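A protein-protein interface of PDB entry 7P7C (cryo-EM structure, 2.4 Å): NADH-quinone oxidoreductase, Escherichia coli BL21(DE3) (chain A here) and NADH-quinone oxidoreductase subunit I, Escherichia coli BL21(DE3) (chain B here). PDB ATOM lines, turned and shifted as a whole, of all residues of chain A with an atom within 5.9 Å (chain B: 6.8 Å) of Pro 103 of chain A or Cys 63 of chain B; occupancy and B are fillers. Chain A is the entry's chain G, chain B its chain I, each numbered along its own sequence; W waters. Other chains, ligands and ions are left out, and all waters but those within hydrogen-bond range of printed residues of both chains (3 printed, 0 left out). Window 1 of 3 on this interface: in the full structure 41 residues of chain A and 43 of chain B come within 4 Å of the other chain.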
ATOM      1  N   HIS A 100       5.290  19.086 -32.323  1.00  0.00           N
ATOM      2  CA  HIS A 100       6.350  18.340 -31.645  1.00  0.00           C
ATOM      3  C   HIS A 100       6.653  18.967 -30.279  1.00  0.00           C
ATOM      4  O   HIS A 100       7.745  19.461 -30.013  1.00  0.00           O
ATOM      5  CB  HIS A 100       7.585  18.315 -32.536  1.00  0.00           C
ATOM      6  CG  HIS A 100       8.555  17.224 -32.217  1.00  0.00           C
ATOM      7  ND1 HIS A 100       8.522  15.995 -32.839  1.00  0.00           N
ATOM      8  CD2 HIS A 100       9.602  17.185 -31.360  1.00  0.00           C
ATOM      9  CE1 HIS A 100       9.499  15.241 -32.368  1.00  0.00           C
ATOM     10  NE2 HIS A 100      10.169  15.940 -31.471  1.00  0.00           N
ATOM     11  N   ASP A 101       5.656  18.927 -29.396  1.00  0.00           N
ATOM     12  CA  ASP A 101       5.621  19.838 -28.263  1.00  0.00           C
ATOM     13  C   ASP A 101       5.699  19.196 -26.886  1.00  0.00           C
ATOM     14  O   ASP A 101       5.827  19.940 -25.911  1.00  0.00           O
ATOM     15  CB  ASP A 101       4.351  20.696 -28.317  1.00  0.00           C
ATOM     16  CG  ASP A 101       4.574  22.028 -28.984  1.00  0.00           C
ATOM     17  OD1 ASP A 101       5.665  22.241 -29.544  1.00  0.00           O
ATOM     18  OD2 ASP A 101       3.654  22.865 -28.942  1.00  0.00           O
ATOM     19  N   CYS A 102       5.633  17.865 -26.775  1.00  0.00           N
ATOM     20  CA  CYS A 102       5.526  17.198 -25.473  1.00  0.00           C
ATOM     21  C   CYS A 102       6.567  17.603 -24.424  1.00  0.00           C
ATOM     22  O   CYS A 102       6.174  17.756 -23.255  1.00  0.00           O
ATOM     23  CB  CYS A 102       5.567  15.670 -25.641  1.00  0.00           C
ATOM     24  SG  CYS A 102       4.232  14.910 -26.551  1.00  0.00           S
ATOM     25  N   PRO A 103       7.867  17.774 -24.732  1.00  0.00           N
ATOM     26  CA  PRO A 103       8.784  18.266 -23.689  1.00  0.00           C
ATOM     27  C   PRO A 103       8.449  19.648 -23.149  1.00  0.00           C
ATOM     28  O   PRO A 103       8.682  19.904 -21.964  1.00  0.00           O
ATOM     29  CB  PRO A 103      10.144  18.260 -24.397  1.00  0.00           C
ATOM     30  CG  PRO A 103      10.013  17.241 -25.426  1.00  0.00           C
ATOM     31  CD  PRO A 103       8.630  17.381 -25.933  1.00  0.00           C
ATOM     32  N   VAL A 104       7.903  20.543 -23.969  1.00  0.00           N
ATOM     33  CA  VAL A 104       7.639  21.910 -23.535  1.00  0.00           C
ATOM     34  C   VAL A 104       6.144  22.152 -23.419  1.00  0.00           C
ATOM     35  O   VAL A 104       5.678  23.288 -23.543  1.00  0.00           O
ATOM     36  CB  VAL A 104       8.277  22.930 -24.492  1.00  0.00           C
ATOM     37  CG1 VAL A 104       9.765  22.991 -24.270  1.00  0.00           C
ATOM     38  CG2 VAL A 104       7.959  22.574 -25.929  1.00  0.00           C
ATOM     39  N   CYS A 105       5.383  21.093 -23.188  1.00  0.00           N
ATOM     40  CA  CYS A 105       3.939  21.183 -23.043  1.00  0.00           C
ATOM     41  C   CYS A 105       3.556  20.786 -21.629  1.00  0.00           C
ATOM     42  O   CYS A 105       3.990  19.743 -21.133  1.00  0.00           O
ATOM     43  CB  CYS A 105       3.236  20.295 -24.061  1.00  0.00           C
ATOM     44  SG  CYS A 105       1.474  20.117 -23.870  1.00  0.00           S
ATOM     45  N   ARG A 216       5.945  18.013 -13.343  1.00  0.00           N
ATOM     46  CA  ARG A 216       5.132  16.952 -13.910  1.00  0.00           C
ATOM     47  C   ARG A 216       4.330  16.243 -12.822  1.00  0.00           C
ATOM     48  O   ARG A 216       4.623  16.348 -11.630  1.00  0.00           O
ATOM     49  CB  ARG A 216       6.014  15.966 -14.663  1.00  0.00           C
ATOM     50  CG  ARG A 216       6.873  16.621 -15.727  1.00  0.00           C
ATOM     51  CD  ARG A 216       6.120  16.744 -17.032  1.00  0.00           C
ATOM     52  NE  ARG A 216       6.961  17.241 -18.108  1.00  0.00           N
ATOM     53  CZ  ARG A 216       6.505  17.826 -19.206  1.00  0.00           C
ATOM     54  NH1 ARG A 216       5.212  18.004 -19.404  1.00  0.00           N
ATOM     55  NH2 ARG A 216       7.369  18.244 -20.124  1.00  0.00           N
ATOM     56  N   TRP A 218       3.915  13.059 -12.036  1.00  0.00           N
ATOM     57  CA  TRP A 218       4.615  12.035 -11.271  1.00  0.00           C
ATOM     58  C   TRP A 218       5.522  12.621 -10.195  1.00  0.00           C
ATOM     59  O   TRP A 218       5.857  11.917  -9.240  1.00  0.00           O
ATOM     60  CB  TRP A 218       5.427  11.140 -12.208  1.00  0.00           C
ATOM     61  CG  TRP A 218       6.473  11.861 -13.020  1.00  0.00           C
ATOM     62  CD1 TRP A 218       7.682  12.314 -12.586  1.00  0.00           C
ATOM     63  CD2 TRP A 218       6.403  12.185 -14.411  1.00  0.00           C
ATOM     64  NE1 TRP A 218       8.360  12.913 -13.611  1.00  0.00           N
ATOM     65  CE2 TRP A 218       7.602  12.840 -14.747  1.00  0.00           C
ATOM     66  CE3 TRP A 218       5.443  11.986 -15.406  1.00  0.00           C
ATOM     67  CZ2 TRP A 218       7.868  13.291 -16.034  1.00  0.00           C
ATOM     68  CZ3 TRP A 218       5.706  12.448 -16.678  1.00  0.00           C
ATOM     69  CH2 TRP A 218       6.908  13.094 -16.980  1.00  0.00           C
ATOM     70  N   CYS B  60      18.674  22.222 -22.962  1.00  0.00           N
ATOM     71  CA  CYS B  60      17.733  21.660 -22.004  1.00  0.00           C
ATOM     72  C   CYS B  60      16.479  22.513 -21.919  1.00  0.00           C
ATOM     73  O   CYS B  60      16.545  23.725 -21.707  1.00  0.00           O
ATOM     74  CB  CYS B  60      18.373  21.525 -20.626  1.00  0.00           C
ATOM     75  SG  CYS B  60      17.246  20.886 -19.376  1.00  0.00           S
ATOM     76  N   VAL B  61      15.331  21.866 -22.100  1.00  0.00           N
ATOM     77  CA  VAL B  61      14.039  22.524 -22.012  1.00  0.00           C
ATOM     78  C   VAL B  61      13.343  22.219 -20.694  1.00  0.00           C
ATOM     79  O   VAL B  61      12.159  22.527 -20.541  1.00  0.00           O
ATOM     80  CB  VAL B  61      13.151  22.139 -23.204  1.00  0.00           C
ATOM     81  CG1 VAL B  61      13.828  22.512 -24.499  1.00  0.00           C
ATOM     82  CG2 VAL B  61      12.834  20.656 -23.176  1.00  0.00           C
ATOM     83  N   ALA B  62      14.058  21.606 -19.745  1.00  0.00           N
ATOM     84  CA  ALA B  62      13.558  21.286 -18.406  1.00  0.00           C
ATOM     85  C   ALA B  62      12.284  20.449 -18.456  1.00  0.00           C
ATOM     86  O   ALA B  62      11.318  20.703 -17.735  1.00  0.00           O
ATOM     87  CB  ALA B  62      13.349  22.549 -17.578  1.00  0.00           C
ATOM     88  N   CYS B  63      12.281  19.444 -19.323  1.00  0.00           N
ATOM     89  CA  CYS B  63      11.112  18.604 -19.518  1.00  0.00           C
ATOM     90  C   CYS B  63      10.979  17.512 -18.468  1.00  0.00           C
ATOM     91  O   CYS B  63       9.945  16.836 -18.442  1.00  0.00           O
ATOM     92  CB  CYS B  63      11.160  17.982 -20.906  1.00  0.00           C
ATOM     93  SG  CYS B  63      12.260  16.587 -21.063  1.00  0.00           S
ATOM     94  N   ASN B  64      12.009  17.312 -17.642  1.00  0.00           N
ATOM     95  CA  ASN B  64      12.032  16.400 -16.498  1.00  0.00           C
ATOM     96  C   ASN B  64      11.949  14.926 -16.880  1.00  0.00           C
ATOM     97  O   ASN B  64      11.661  14.091 -16.022  1.00  0.00           O
ATOM     98  CB  ASN B  64      10.926  16.727 -15.487  1.00  0.00           C
ATOM     99  CG  ASN B  64      11.452  17.421 -14.266  1.00  0.00           C
ATOM    100  OD1 ASN B  64      12.140  16.819 -13.447  1.00  0.00           O
ATOM    101  ND2 ASN B  64      11.135  18.698 -14.131  1.00  0.00           N
ATOM    102  N   LEU B  65      12.213  14.569 -18.137  1.00  0.00           N
ATOM    103  CA  LEU B  65      12.199  13.157 -18.511  1.00  0.00           C
ATOM    104  C   LEU B  65      13.423  12.414 -17.979  1.00  0.00           C
ATOM    105  O   LEU B  65      13.324  11.240 -17.608  1.00  0.00           O
ATOM    106  CB  LEU B  65      12.112  13.011 -20.028  1.00  0.00           C
ATOM    107  CG  LEU B  65      10.753  13.276 -20.676  1.00  0.00           C
ATOM    108  CD1 LEU B  65      10.819  12.988 -22.163  1.00  0.00           C
ATOM    109  CD2 LEU B  65       9.660  12.460 -20.015  1.00  0.00           C
ATOM    110  N   CYS B  66      14.583  13.076 -17.944  1.00  0.00           N
ATOM    111  CA  CYS B  66      15.794  12.425 -17.453  1.00  0.00           C
ATOM    112  C   CYS B  66      15.707  12.129 -15.962  1.00  0.00           C
ATOM    113  O   CYS B  66      16.219  11.104 -15.500  1.00  0.00           O
ATOM    114  CB  CYS B  66      17.019  13.289 -17.743  1.00  0.00           C
ATOM    115  SG  CYS B  66      16.968  14.923 -16.998  1.00  0.00           S
ATOM    116  N   VAL B  68      12.957  11.492 -14.117  1.00  0.00           N
ATOM    117  CA  VAL B  68      12.081  10.359 -13.850  1.00  0.00           C
ATOM    118  C   VAL B  68      12.653   9.077 -14.449  1.00  0.00           C
ATOM    119  O   VAL B  68      12.425   7.987 -13.918  1.00  0.00           O
ATOM    120  CB  VAL B  68      10.655  10.669 -14.347  1.00  0.00           C
ATOM    121  CG1 VAL B  68      10.618  10.880 -15.843  1.00  0.00           C
ATOM    122  CG2 VAL B  68       9.660   9.606 -13.905  1.00  0.00           C
ATOM    123  N   LEU B  77      15.700  19.088 -10.956  1.00  0.00           N
ATOM    124  CA  LEU B  77      15.676  20.301 -11.757  1.00  0.00           C
ATOM    125  C   LEU B  77      14.311  20.957 -11.629  1.00  0.00           C
ATOM    126  O   LEU B  77      13.347  20.339 -11.173  1.00  0.00           O
ATOM    127  CB  LEU B  77      16.002  20.004 -13.224  1.00  0.00           C
ATOM    128  CG  LEU B  77      14.995  19.122 -13.960  1.00  0.00           C
ATOM    129  CD1 LEU B  77      14.446  19.859 -15.149  1.00  0.00           C
ATOM    130  CD2 LEU B  77      15.619  17.811 -14.387  1.00  0.00           C
ATOM    131  N   LYS B  79      11.729  23.739 -13.932  1.00  0.00           N
ATOM    132  CA  LYS B  79      11.489  24.479 -15.160  1.00  0.00           C
ATOM    133  C   LYS B  79      11.295  25.962 -14.875  1.00  0.00           C
ATOM    134  O   LYS B  79      10.584  26.339 -13.940  1.00  0.00           O
ATOM    135  CB  LYS B  79      10.269  23.913 -15.884  1.00  0.00           C
ATOM    136  CG  LYS B  79       9.830  24.708 -17.099  1.00  0.00           C
ATOM    137  CD  LYS B  79       8.467  25.338 -16.885  1.00  0.00           C
ATOM    138  CE  LYS B  79       8.209  26.443 -17.884  1.00  0.00           C
ATOM    139  NZ  LYS B  79       6.892  27.092 -17.675  1.00  0.00           N
ATOM    140  N   TRP B  87      11.417  27.425 -22.634  1.00  0.00           N
ATOM    141  CA  TRP B  87      11.650  26.669 -21.413  1.00  0.00           C
ATOM    142  C   TRP B  87      13.140  26.418 -21.218  1.00  0.00           C
ATOM    143  O   TRP B  87      13.889  26.223 -22.176  1.00  0.00           O
ATOM    144  CB  TRP B  87      10.921  25.329 -21.460  1.00  0.00           C
ATOM    145  CG  TRP B  87       9.436  25.370 -21.297  1.00  0.00           C
ATOM    146  CD1 TRP B  87       8.592  26.377 -21.655  1.00  0.00           C
ATOM    147  CD2 TRP B  87       8.614  24.332 -20.757  1.00  0.00           C
ATOM    148  NE1 TRP B  87       7.298  26.036 -21.360  1.00  0.00           N
ATOM    149  CE2 TRP B  87       7.285  24.783 -20.808  1.00  0.00           C
ATOM    150  CE3 TRP B  87       8.876  23.065 -20.227  1.00  0.00           C
ATOM    151  CZ2 TRP B  87       6.222  24.016 -20.348  1.00  0.00           C
ATOM    152  CZ3 TRP B  87       7.820  22.306 -19.773  1.00  0.00           C
ATOM    153  CH2 TRP B  87       6.509  22.782 -19.837  1.00  0.00           C
ATOM    154  N   ALA B 108      16.875   8.994 -22.443  1.00  0.00           N
ATOM    155  CA  ALA B 108      15.550   9.572 -22.294  1.00  0.00           C
ATOM    156  C   ALA B 108      15.453  11.016 -22.763  1.00  0.00           C
ATOM    157  O   ALA B 108      14.334  11.519 -22.898  1.00  0.00           O
ATOM    158  CB  ALA B 108      15.103   9.499 -20.838  1.00  0.00           C
ATOM    159  N   CYS B 109      16.567  11.691 -23.006  1.00  0.00           N
ATOM    160  CA  CYS B 109      16.519  13.113 -23.326  1.00  0.00           C
ATOM    161  C   CYS B 109      15.991  13.332 -24.734  1.00  0.00           C
ATOM    162  O   CYS B 109      16.589  12.836 -25.693  1.00  0.00           O
ATOM    163  CB  CYS B 109      17.892  13.748 -23.189  1.00  0.00           C
ATOM    164  SG  CYS B 109      17.928  15.555 -23.354  1.00  0.00           S
ATOM    165  N   PRO B 110      14.897  14.071 -24.909  1.00  0.00           N
ATOM    166  CA  PRO B 110      14.367  14.337 -26.249  1.00  0.00           C
ATOM    167  C   PRO B 110      14.994  15.528 -26.957  1.00  0.00           C
ATOM    168  O   PRO B 110      14.569  15.848 -28.071  1.00  0.00           O
ATOM    169  CB  PRO B 110      12.884  14.597 -25.962  1.00  0.00           C
ATOM    170  CG  PRO B 110      12.874  15.190 -24.604  1.00  0.00           C
ATOM    171  CD  PRO B 110      14.059  14.663 -23.854  1.00  0.00           C
ATOM    172  N   THR B 111      15.964  16.202 -26.344  1.00  0.00           N
ATOM    173  CA  THR B 111      16.627  17.342 -26.958  1.00  0.00           C
ATOM    174  C   THR B 111      18.122  17.132 -27.152  1.00  0.00           C
ATOM    175  O   THR B 111      18.785  18.028 -27.685  1.00  0.00           O
ATOM    176  CB  THR B 111      16.410  18.614 -26.123  1.00  0.00           C
ATOM    177  OG1 THR B 111      17.239  18.569 -24.961  1.00  0.00           O
ATOM    178  CG2 THR B 111      14.962  18.752 -25.687  1.00  0.00           C
ATOM    179  N   PHE B 150      16.080  20.973 -30.793  1.00  0.00           N
ATOM    180  CA  PHE B 150      14.688  20.628 -30.518  1.00  0.00           C
ATOM    181  C   PHE B 150      13.754  21.777 -30.864  1.00  0.00           C
ATOM    182  O   PHE B 150      12.645  21.554 -31.357  1.00  0.00           O
ATOM    183  CB  PHE B 150      14.514  20.232 -29.050  1.00  0.00           C
ATOM    184  CG  PHE B 150      13.075  20.153 -28.607  1.00  0.00           C
ATOM    185  CD1 PHE B 150      12.298  19.059 -28.940  1.00  0.00           C
ATOM    186  CD2 PHE B 150      12.505  21.170 -27.857  1.00  0.00           C
ATOM    187  CE1 PHE B 150      10.978  18.981 -28.539  1.00  0.00           C
ATOM    188  CE2 PHE B 150      11.188  21.099 -27.458  1.00  0.00           C
ATOM    189  CZ  PHE B 150      10.424  20.001 -27.798  1.00  0.00           C
HETATM  190  O   HOH W   1      12.492  15.759 -29.846  1.00  0.00           O
HETATM  191  O   HOH W   2       8.640  17.609 -12.765  1.00  0.00           O
HETATM  192  O   HOH W   3      10.794  14.016 -13.223  1.00  0.00           O
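Printed residues of chain A that touch a printed residue of chain B: His 100, Pro 103, Val 104, Cys 105, Arg 216 and Trp 218.
Hydrophobic or aromatic side chains of chain A within 4 Å of the printed part of chain B: His 100, Pro 103, Val 104 and Trp 218.
Of the 16 printed residues of chain B, 7 touch a printed residue of chain A.
Hydrophobic or aromatic side chains of chain B within 4 Å of the printed part of chain A: Val 61, Val 68, Trp 87, Pro 110 and Phe 150.
O of Cys 105 of chain A lies within hydrogen-bond range of NH1 of Arg 216 of chain A (2.7 Å).
O of Pro 103 of chain A sits at hydrogen-bond distance from NH2 of Arg 216 of chain A (2.8 Å).
The side-chain sulfur of Cys 63 of chain B sits close to the backbone NH of Leu 65 of chain B.
The backbone carbonyl oxygen of Cys 102 of chain A sits at hydrogen-bond distance from the guanidinium group of Arg 216 of chain A (3.4 Å).
Water W3 lies within hydrogen-bond range of NE1 of Trp 218 of chain A (2.7 Å), O of Asn 64 of chain B (2.9 Å) and N of Val 68 of chain B (3.4 Å).
Water W1 lies within hydrogen-bond range of O of Pro 110 of chain B and NE2 of His 100 of chain A.
Water W2 bridges N of Arg 216 of chain A (2.8 Å) and ND2 of Asn 64 of chain B (3.0 Å).
Pro 103 of chain A touches just these residues of chain B: Val 61, Cys 63, Trp 87, Pro 110 and Phe 150.
Cys 60 of chain B touches none of the printed residues of chain A.
Printed residues of chain A within 4 Å of Val 61 of chain B: Pro 103 (3.8 Å) and Val 104 (3.7 Å).
Cys 63 of chain B touches just these residues of chain A: Pro 103 and Arg 216.
Of the printed residues of chain A, Asn 64 of chain B touches Trp 218.
Of the printed residues of chain A, Pro 110 of chain B touches Pro 103 (3.6 Å).
Printed residues of chain A within 4 Å of Phe 150 of chain B: His 100 (3.5 Å), Pro 103 (3.7 Å) and Val 104 (3.9 Å).
Among the printed residues, pairs that only touch across the chains: His 100 of chain A with Phe 150 of chain B, Pro 103 of chain A with Val 61 of chain B, Pro 103 of chain A with Cys 63 of chain B, Pro 103 of chain A with Trp 87 of chain B, Pro 103 of chain A with Pro 110 of chain B, Pro 103 of chain A with Phe 150 of chain B, Val 104 of chain A with Val 61 of chain B, Val 104 of chain A with Trp 87 of chain B, Val 104 of chain A with Phe 150 of chain B, Cys 105 of chain A with Trp 87 of chain B, Trp 218 of chain A with Asn 64 of chain B and Trp 218 of chain A with Val 68 of chain B.
NE of Arg 216 of chain A is in hydrogen-bond range of O of Cys 63 of chain B (3.0 Å).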
